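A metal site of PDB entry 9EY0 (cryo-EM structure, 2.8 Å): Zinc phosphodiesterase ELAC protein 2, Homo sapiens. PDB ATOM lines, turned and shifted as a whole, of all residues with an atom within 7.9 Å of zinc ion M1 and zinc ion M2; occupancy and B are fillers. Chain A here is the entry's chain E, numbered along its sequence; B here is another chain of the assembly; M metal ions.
Residues that only touch zinc ion M1: Ser 461 (3.4 Å). Of the 27 residues printed, 5 come within 4 Å of zinc ion M1. Along chain A the residues within 4 Å of zinc ion M1 span positions 461 to 695.
OD2 of Asp 637 binds zinc ion M1, 2.0 Å away. OD2 of Asp 521 is bound to zinc ion M1. NE2 of His 522 binds zinc ion M1, at 2.0 Å. NE2 of His 695 is bound to zinc ion M1, at 2.0 Å. Slightly farther from zinc ion M1 lies OD1 of Asp 637 (2.8 Å).
Zinc ion M2 is bound by OD2 of Asp 637 (2.0 Å). A ring nitrogen (NE2) of His 517 binds zinc ion M2. Zinc ion M2 is bound by ND1 of His 519. NE2 of His 615 binds zinc ion M2, 2.0 Å away.
Four residues have an atom within 4 Å of zinc ion M2: His 517, His 519, His 615 and Asp 637. Along chain A the residues within 4 Å of zinc ion M2 span positions 517 to 637. The nearest printed residue that does not touch zinc ion M2 is His 522 (4.02 Å).
The backbone carbonyl oxygen of Thr 672 lies within hydrogen-bond range of a ring nitrogen (ND1) of His 615 (2.9 Å). The side-chain hydroxyl of Thr 659 lies within hydrogen-bond range of the backbone carbonyl oxygen of His 695 (2.9 Å). A ring nitrogen (ND1) of His 695 lies within hydrogen-bond range of the side-chain carboxylate (OE2) of Glu 657 (3.3 Å). O of Ser 461 lies close to NE2 of His 695 (3.5 Å). The side-chain hydroxyl (OG) of Ser 516 lies within hydrogen-bond range of a ring nitrogen (ND1) of His 517 (2.9 Å). OP2 of C 68 of chain B is in hydrogen-bond range of the side-chain hydroxyl (OG) of Ser 461, at 3.2 Å. The side-chain carboxylate of Asp 486 lies within hydrogen-bond range of a ring nitrogen (ND1) of His 522.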
ATOM      1  N   GLY A 460      -0.230 -18.804  19.768  1.00  0.00           N
ATOM      2  CA  GLY A 460      -1.579 -18.305  19.918  1.00  0.00           C
ATOM      3  C   GLY A 460      -2.552 -19.382  20.346  1.00  0.00           C
ATOM      4  O   GLY A 460      -2.284 -20.575  20.245  1.00  0.00           O
ATOM      5  N   SER A 461      -3.719 -18.944  20.820  1.00  0.00           N
ATOM      6  CA  SER A 461      -4.748 -19.848  21.308  1.00  0.00           C
ATOM      7  C   SER A 461      -5.861 -20.064  20.278  1.00  0.00           C
ATOM      8  O   SER A 461      -6.092 -21.200  19.849  1.00  0.00           O
ATOM      9  CB  SER A 461      -5.350 -19.303  22.622  1.00  0.00           C
ATOM     10  OG  SER A 461      -5.874 -17.999  22.438  1.00  0.00           O
ATOM     11  N   ALA A 462      -6.550 -19.000  19.887  1.00  0.00           N
ATOM     12  CA  ALA A 462      -7.686 -19.105  18.981  1.00  0.00           C
ATOM     13  C   ALA A 462      -7.475 -18.367  17.664  1.00  0.00           C
ATOM     14  O   ALA A 462      -7.734 -18.943  16.604  1.00  0.00           O
ATOM     15  CB  ALA A 462      -8.946 -18.563  19.677  1.00  0.00           C
ATOM     16  N   VAL A 470      -1.198 -18.211  15.812  1.00  0.00           N
ATOM     17  CA  VAL A 470      -1.782 -19.464  16.253  1.00  0.00           C
ATOM     18  C   VAL A 470      -0.683 -20.517  16.420  1.00  0.00           C
ATOM     19  O   VAL A 470       0.404 -20.416  15.850  1.00  0.00           O
ATOM     20  CB  VAL A 470      -2.864 -19.964  15.277  1.00  0.00           C
ATOM     21  CG1 VAL A 470      -4.123 -19.113  15.414  1.00  0.00           C
ATOM     22  CG2 VAL A 470      -2.356 -19.926  13.846  1.00  0.00           C
ATOM     23  N   SER A 471      -0.990 -21.539  17.222  1.00  0.00           N
ATOM     24  CA  SER A 471       0.025 -22.500  17.629  1.00  0.00           C
ATOM     25  C   SER A 471       0.675 -23.168  16.418  1.00  0.00           C
ATOM     26  O   SER A 471      -0.006 -23.646  15.509  1.00  0.00           O
ATOM     27  CB  SER A 471      -0.596 -23.562  18.532  1.00  0.00           C
ATOM     28  OG  SER A 471       0.392 -24.425  19.068  1.00  0.00           O
ATOM     29  N   ASP A 486       2.606 -28.656  14.760  1.00  0.00           N
ATOM     30  CA  ASP A 486       1.275 -28.094  14.551  1.00  0.00           C
ATOM     31  C   ASP A 486       1.352 -27.108  13.389  1.00  0.00           C
ATOM     32  O   ASP A 486       2.405 -26.523  13.125  1.00  0.00           O
ATOM     33  CB  ASP A 486       0.743 -27.414  15.819  1.00  0.00           C
ATOM     34  CG  ASP A 486      -0.388 -28.174  16.468  1.00  0.00           C
ATOM     35  OD1 ASP A 486      -0.567 -28.037  17.694  1.00  0.00           O
ATOM     36  OD2 ASP A 486      -1.103 -28.914  15.765  1.00  0.00           O
ATOM     37  N   SER A 516      -2.680 -31.832  16.418  1.00  0.00           N
ATOM     38  CA  SER A 516      -3.203 -32.263  17.709  1.00  0.00           C
ATOM     39  C   SER A 516      -4.673 -32.632  17.610  1.00  0.00           C
ATOM     40  O   SER A 516      -5.090 -33.720  18.052  1.00  0.00           O
ATOM     41  CB  SER A 516      -2.997 -31.171  18.751  1.00  0.00           C
ATOM     42  OG  SER A 516      -3.745 -31.428  19.929  1.00  0.00           O
ATOM     43  N   HIS A 517      -5.480 -31.760  17.024  1.00  0.00           N
ATOM     44  CA  HIS A 517      -6.909 -32.012  16.853  1.00  0.00           C
ATOM     45  C   HIS A 517      -7.417 -31.143  15.712  1.00  0.00           C
ATOM     46  O   HIS A 517      -6.640 -30.520  14.986  1.00  0.00           O
ATOM     47  CB  HIS A 517      -7.661 -31.769  18.175  1.00  0.00           C
ATOM     48  CG  HIS A 517      -7.392 -30.441  18.794  1.00  0.00           C
ATOM     49  ND1 HIS A 517      -6.144 -30.056  19.226  1.00  0.00           N
ATOM     50  CD2 HIS A 517      -8.221 -29.402  19.067  1.00  0.00           C
ATOM     51  CE1 HIS A 517      -6.206 -28.832  19.731  1.00  0.00           C
ATOM     52  NE2 HIS A 517      -7.462 -28.416  19.649  1.00  0.00           N
ATOM     53  N   LEU A 518      -8.743 -31.079  15.566  1.00  0.00           N
ATOM     54  CA  LEU A 518      -9.373 -30.440  14.414  1.00  0.00           C
ATOM     55  C   LEU A 518      -9.721 -28.980  14.642  1.00  0.00           C
ATOM     56  O   LEU A 518     -10.373 -28.369  13.799  1.00  0.00           O
ATOM     57  CB  LEU A 518     -10.637 -31.222  14.020  1.00  0.00           C
ATOM     58  CG  LEU A 518     -10.509 -32.422  13.068  1.00  0.00           C
ATOM     59  CD1 LEU A 518     -11.845 -32.699  12.395  1.00  0.00           C
ATOM     60  CD2 LEU A 518      -9.420 -32.228  12.015  1.00  0.00           C
ATOM     61  N   HIS A 519      -9.303 -28.399  15.775  1.00  0.00           N
ATOM     62  CA  HIS A 519      -9.541 -26.979  15.994  1.00  0.00           C
ATOM     63  C   HIS A 519      -8.887 -26.162  14.886  1.00  0.00           C
ATOM     64  O   HIS A 519      -7.781 -26.477  14.430  1.00  0.00           O
ATOM     65  CB  HIS A 519      -9.000 -26.553  17.359  1.00  0.00           C
ATOM     66  CG  HIS A 519      -9.973 -26.769  18.483  1.00  0.00           C
ATOM     67  ND1 HIS A 519      -9.585 -26.744  19.814  1.00  0.00           N
ATOM     68  CD2 HIS A 519     -11.304 -27.014  18.490  1.00  0.00           C
ATOM     69  CE1 HIS A 519     -10.636 -26.955  20.580  1.00  0.00           C
ATOM     70  NE2 HIS A 519     -11.692 -27.128  19.798  1.00  0.00           N
ATOM     71  N   ALA A 520      -9.571 -25.099  14.462  1.00  0.00           N
ATOM     72  CA  ALA A 520      -9.090 -24.303  13.343  1.00  0.00           C
ATOM     73  C   ALA A 520      -7.709 -23.725  13.617  1.00  0.00           C
ATOM     74  O   ALA A 520      -6.955 -23.466  12.670  1.00  0.00           O
ATOM     75  CB  ALA A 520     -10.081 -23.185  13.020  1.00  0.00           C
ATOM     76  N   ASP A 521      -7.360 -23.515  14.882  1.00  0.00           N
ATOM     77  CA  ASP A 521      -6.075 -22.937  15.250  1.00  0.00           C
ATOM     78  C   ASP A 521      -4.947 -23.961  15.284  1.00  0.00           C
ATOM     79  O   ASP A 521      -3.892 -23.663  15.855  1.00  0.00           O
ATOM     80  CB  ASP A 521      -6.181 -22.234  16.607  1.00  0.00           C
ATOM     81  CG  ASP A 521      -6.663 -23.164  17.711  1.00  0.00           C
ATOM     82  OD1 ASP A 521      -7.886 -23.387  17.811  1.00  0.00           O
ATOM     83  OD2 ASP A 521      -5.808 -23.668  18.472  1.00  0.00           O
ATOM     84  N   HIS A 522      -5.131 -25.137  14.689  1.00  0.00           N
ATOM     85  CA  HIS A 522      -4.104 -26.175  14.691  1.00  0.00           C
ATOM     86  C   HIS A 522      -3.872 -26.834  13.342  1.00  0.00           C
ATOM     87  O   HIS A 522      -2.821 -27.451  13.164  1.00  0.00           O
ATOM     88  CB  HIS A 522      -4.459 -27.271  15.712  1.00  0.00           C
ATOM     89  CG  HIS A 522      -4.460 -26.791  17.132  1.00  0.00           C
ATOM     90  ND1 HIS A 522      -3.379 -26.955  17.971  1.00  0.00           N
ATOM     91  CD2 HIS A 522      -5.420 -26.160  17.848  1.00  0.00           C
ATOM     92  CE1 HIS A 522      -3.671 -26.440  19.151  1.00  0.00           C
ATOM     93  NE2 HIS A 522      -4.901 -25.949  19.112  1.00  0.00           N
ATOM     94  N   HIS A 615      -9.426 -33.229  25.967  1.00  0.00           N
ATOM     95  CA  HIS A 615      -9.858 -32.111  25.136  1.00  0.00           C
ATOM     96  C   HIS A 615     -11.078 -32.562  24.351  1.00  0.00           C
ATOM     97  O   HIS A 615     -11.717 -33.570  24.688  1.00  0.00           O
ATOM     98  CB  HIS A 615      -8.692 -31.633  24.255  1.00  0.00           C
ATOM     99  CG  HIS A 615      -8.861 -30.232  23.726  1.00  0.00           C
ATOM    100  ND1 HIS A 615      -9.148 -29.172  24.536  1.00  0.00           N
ATOM    101  CD2 HIS A 615      -8.804 -29.751  22.464  1.00  0.00           C
ATOM    102  CE1 HIS A 615      -9.246 -28.073  23.797  1.00  0.00           C
ATOM    103  NE2 HIS A 615      -9.043 -28.401  22.539  1.00  0.00           N
ATOM    104  N   CYS A 616     -11.420 -31.834  23.284  1.00  0.00           N
ATOM    105  CA  CYS A 616     -12.530 -32.216  22.429  1.00  0.00           C
ATOM    106  C   CYS A 616     -12.309 -33.612  21.868  1.00  0.00           C
ATOM    107  O   CYS A 616     -11.203 -34.158  21.947  1.00  0.00           O
ATOM    108  CB  CYS A 616     -12.701 -31.202  21.296  1.00  0.00           C
ATOM    109  SG  CYS A 616     -11.331 -31.178  20.116  1.00  0.00           S
ATOM    110  N   ALA A 619      -8.921 -35.859  20.130  1.00  0.00           N
ATOM    111  CA  ALA A 619      -7.788 -34.996  20.414  1.00  0.00           C
ATOM    112  C   ALA A 619      -6.609 -35.862  20.863  1.00  0.00           C
ATOM    113  O   ALA A 619      -6.769 -36.728  21.723  1.00  0.00           O
ATOM    114  CB  ALA A 619      -8.126 -33.965  21.487  1.00  0.00           C
ATOM    115  N   TYR A 634       5.189 -33.355  23.268  1.00  0.00           N
ATOM    116  CA  TYR A 634       4.338 -32.230  22.916  1.00  0.00           C
ATOM    117  C   TYR A 634       2.891 -32.580  23.240  1.00  0.00           C
ATOM    118  O   TYR A 634       2.416 -33.659  22.892  1.00  0.00           O
ATOM    119  CB  TYR A 634       4.468 -31.878  21.430  1.00  0.00           C
ATOM    120  CG  TYR A 634       3.448 -30.865  20.956  1.00  0.00           C
ATOM    121  CD1 TYR A 634       3.666 -29.506  21.129  1.00  0.00           C
ATOM    122  CD2 TYR A 634       2.260 -31.272  20.351  1.00  0.00           C
ATOM    123  CE1 TYR A 634       2.730 -28.575  20.696  1.00  0.00           C
ATOM    124  CE2 TYR A 634       1.328 -30.348  19.922  1.00  0.00           C
ATOM    125  CZ  TYR A 634       1.565 -29.001  20.101  1.00  0.00           C
ATOM    126  OH  TYR A 634       0.638 -28.085  19.675  1.00  0.00           O
ATOM    127  N   GLY A 636      -0.989 -30.907  22.836  1.00  0.00           N
ATOM    128  CA  GLY A 636      -1.816 -29.861  22.268  1.00  0.00           C
ATOM    129  C   GLY A 636      -2.735 -29.261  23.309  1.00  0.00           C
ATOM    130  O   GLY A 636      -2.396 -29.236  24.494  1.00  0.00           O
ATOM    131  N   ASP A 637      -3.891 -28.761  22.885  1.00  0.00           N
ATOM    132  CA  ASP A 637      -4.883 -28.252  23.831  1.00  0.00           C
ATOM    133  C   ASP A 637      -5.356 -29.389  24.710  1.00  0.00           C
ATOM    134  O   ASP A 637      -5.916 -30.376  24.217  1.00  0.00           O
ATOM    135  CB  ASP A 637      -6.053 -27.626  23.063  1.00  0.00           C
ATOM    136  CG  ASP A 637      -5.603 -26.574  22.067  1.00  0.00           C
ATOM    137  OD1 ASP A 637      -4.408 -26.213  22.078  1.00  0.00           O
ATOM    138  OD2 ASP A 637      -6.455 -26.107  21.279  1.00  0.00           O
ATOM    139  N   THR A 638      -5.137 -29.287  26.019  1.00  0.00           N
ATOM    140  CA  THR A 638      -5.489 -30.359  26.930  1.00  0.00           C
ATOM    141  C   THR A 638      -5.551 -29.846  28.365  1.00  0.00           C
ATOM    142  O   THR A 638      -4.850 -28.894  28.717  1.00  0.00           O
ATOM    143  CB  THR A 638      -4.485 -31.513  26.852  1.00  0.00           C
ATOM    144  OG1 THR A 638      -4.846 -32.533  27.804  1.00  0.00           O
ATOM    145  CG2 THR A 638      -3.073 -31.027  27.158  1.00  0.00           C
ATOM    146  N   GLU A 657       0.465 -26.823  27.147  1.00  0.00           N
ATOM    147  CA  GLU A 657      -0.399 -25.660  27.020  1.00  0.00           C
ATOM    148  C   GLU A 657      -0.471 -24.902  28.343  1.00  0.00           C
ATOM    149  O   GLU A 657      -0.548 -25.501  29.416  1.00  0.00           O
ATOM    150  CB  GLU A 657      -1.796 -26.093  26.569  1.00  0.00           C
ATOM    151  CG  GLU A 657      -2.915 -25.114  26.897  1.00  0.00           C
ATOM    152  CD  GLU A 657      -4.288 -25.692  26.613  1.00  0.00           C
ATOM    153  OE1 GLU A 657      -4.817 -26.423  27.457  1.00  0.00           O
ATOM    154  OE2 GLU A 657      -4.830 -25.400  25.525  1.00  0.00           O
ATOM    155  N   THR A 659      -2.715 -21.936  28.505  1.00  0.00           N
ATOM    156  CA  THR A 659      -3.630 -20.934  27.953  1.00  0.00           C
ATOM    157  C   THR A 659      -4.047 -19.912  29.004  1.00  0.00           C
ATOM    158  O   THR A 659      -3.974 -18.704  28.765  1.00  0.00           O
ATOM    159  CB  THR A 659      -4.865 -21.639  27.371  1.00  0.00           C
ATOM    160  OG1 THR A 659      -4.459 -22.527  26.324  1.00  0.00           O
ATOM    161  CG2 THR A 659      -5.838 -20.616  26.807  1.00  0.00           C
ATOM    162  N   LYS A 671     -13.644 -24.416  29.141  1.00  0.00           N
ATOM    163  CA  LYS A 671     -12.885 -24.245  27.904  1.00  0.00           C
ATOM    164  C   LYS A 671     -11.975 -25.427  27.602  1.00  0.00           C
ATOM    165  O   LYS A 671     -11.350 -25.446  26.533  1.00  0.00           O
ATOM    166  CB  LYS A 671     -12.045 -22.970  27.995  1.00  0.00           C
ATOM    167  CG  LYS A 671     -12.868 -21.696  28.094  1.00  0.00           C
ATOM    168  CD  LYS A 671     -11.991 -20.474  28.365  1.00  0.00           C
ATOM    169  CE  LYS A 671     -12.746 -19.183  28.130  1.00  0.00           C
ATOM    170  NZ  LYS A 671     -13.020 -18.942  26.684  1.00  0.00           N
ATOM    171  N   THR A 672     -11.897 -26.412  28.497  1.00  0.00           N
ATOM    172  CA  THR A 672     -11.066 -27.605  28.295  1.00  0.00           C
ATOM    173  C   THR A 672      -9.617 -27.225  28.002  1.00  0.00           C
ATOM    174  O   THR A 672      -9.068 -27.493  26.933  1.00  0.00           O
ATOM    175  CB  THR A 672     -11.635 -28.504  27.189  1.00  0.00           C
ATOM    176  OG1 THR A 672     -12.069 -27.700  26.082  1.00  0.00           O
ATOM    177  CG2 THR A 672     -12.803 -29.325  27.709  1.00  0.00           C
ATOM    178  N   HIS A 673      -8.986 -26.577  28.985  1.00  0.00           N
ATOM    179  CA  HIS A 673      -7.593 -26.174  28.887  1.00  0.00           C
ATOM    180  C   HIS A 673      -6.952 -26.295  30.254  1.00  0.00           C
ATOM    181  O   HIS A 673      -7.565 -26.779  31.213  1.00  0.00           O
ATOM    182  CB  HIS A 673      -7.472 -24.750  28.331  1.00  0.00           C
ATOM    183  CG  HIS A 673      -7.902 -24.619  26.905  1.00  0.00           C
ATOM    184  ND1 HIS A 673      -7.326 -25.343  25.880  1.00  0.00           N
ATOM    185  CD2 HIS A 673      -8.861 -23.850  26.325  1.00  0.00           C
ATOM    186  CE1 HIS A 673      -7.903 -25.025  24.735  1.00  0.00           C
ATOM    187  NE2 HIS A 673      -8.836 -24.127  24.978  1.00  0.00           N
ATOM    188  N   HIS A 695       0.839 -21.934  23.469  1.00  0.00           N
ATOM    189  CA  HIS A 695      -0.610 -21.889  23.282  1.00  0.00           C
ATOM    190  C   HIS A 695      -1.263 -20.952  24.293  1.00  0.00           C
ATOM    191  O   HIS A 695      -2.327 -21.240  24.840  1.00  0.00           O
ATOM    192  CB  HIS A 695      -1.224 -23.294  23.373  1.00  0.00           C
ATOM    193  CG  HIS A 695      -2.559 -23.411  22.715  1.00  0.00           C
ATOM    194  ND1 HIS A 695      -3.738 -23.111  23.361  1.00  0.00           N
ATOM    195  CD2 HIS A 695      -2.914 -23.786  21.458  1.00  0.00           C
ATOM    196  CE1 HIS A 695      -4.755 -23.303  22.546  1.00  0.00           C
ATOM    197  NE2 HIS A 695      -4.277 -23.711  21.382  1.00  0.00           N
ATOM    198  P     C B  68      -9.465 -17.492  24.575  1.00  0.00           P
ATOM    199  OP1   C B  68     -10.236 -17.635  25.831  1.00  0.00           O
ATOM    200  OP2   C B  68      -8.027 -17.101  24.630  1.00  0.00           O
ATOM    201  O5'   C B  68      -9.570 -18.871  23.780  1.00  0.00           O
ATOM    202  C5'   C B  68      -9.175 -20.083  24.388  1.00  0.00           C
ATOM    203  C4'   C B  68     -10.175 -21.181  24.109  1.00  0.00           C
ATOM    204  O4'   C B  68     -11.508 -20.732  24.447  1.00  0.00           O
ATOM    205  C3'   C B  68     -10.295 -21.634  22.658  1.00  0.00           C
ATOM    206  O3'   C B  68      -9.272 -22.537  22.268  1.00  0.00           O
ATOM    207  C2'   C B  68     -11.691 -22.235  22.615  1.00  0.00           C
ATOM    208  O2'   C B  68     -11.700 -23.555  23.140  1.00  0.00           O
ATOM    209  C1'   C B  68     -12.455 -21.305  23.568  1.00  0.00           C
ATOM    210  N1    C B  68     -13.149 -20.216  22.845  1.00  0.00           N
ATOM    211  C2    C B  68     -14.394 -20.480  22.270  1.00  0.00           C
ATOM    212  O2    C B  68     -14.880 -21.620  22.379  1.00  0.00           O
ATOM    213  N3    C B  68     -15.044 -19.498  21.610  1.00  0.00           N
ATOM    214  C4    C B  68     -14.482 -18.284  21.504  1.00  0.00           C
ATOM    215  N4    C B  68     -15.157 -17.341  20.849  1.00  0.00           N
ATOM    216  C5    C B  68     -13.216 -17.991  22.089  1.00  0.00           C
ATOM    217  C6    C B  68     -12.588 -18.978  22.739  1.00  0.00           C
HETATM  218 ZN    ZN M   1      -5.777 -24.532  20.266  1.00  0.00          ZN
HETATM  219 ZN    ZN M   2      -8.118 -27.214  21.155  1.00  0.00          ZN
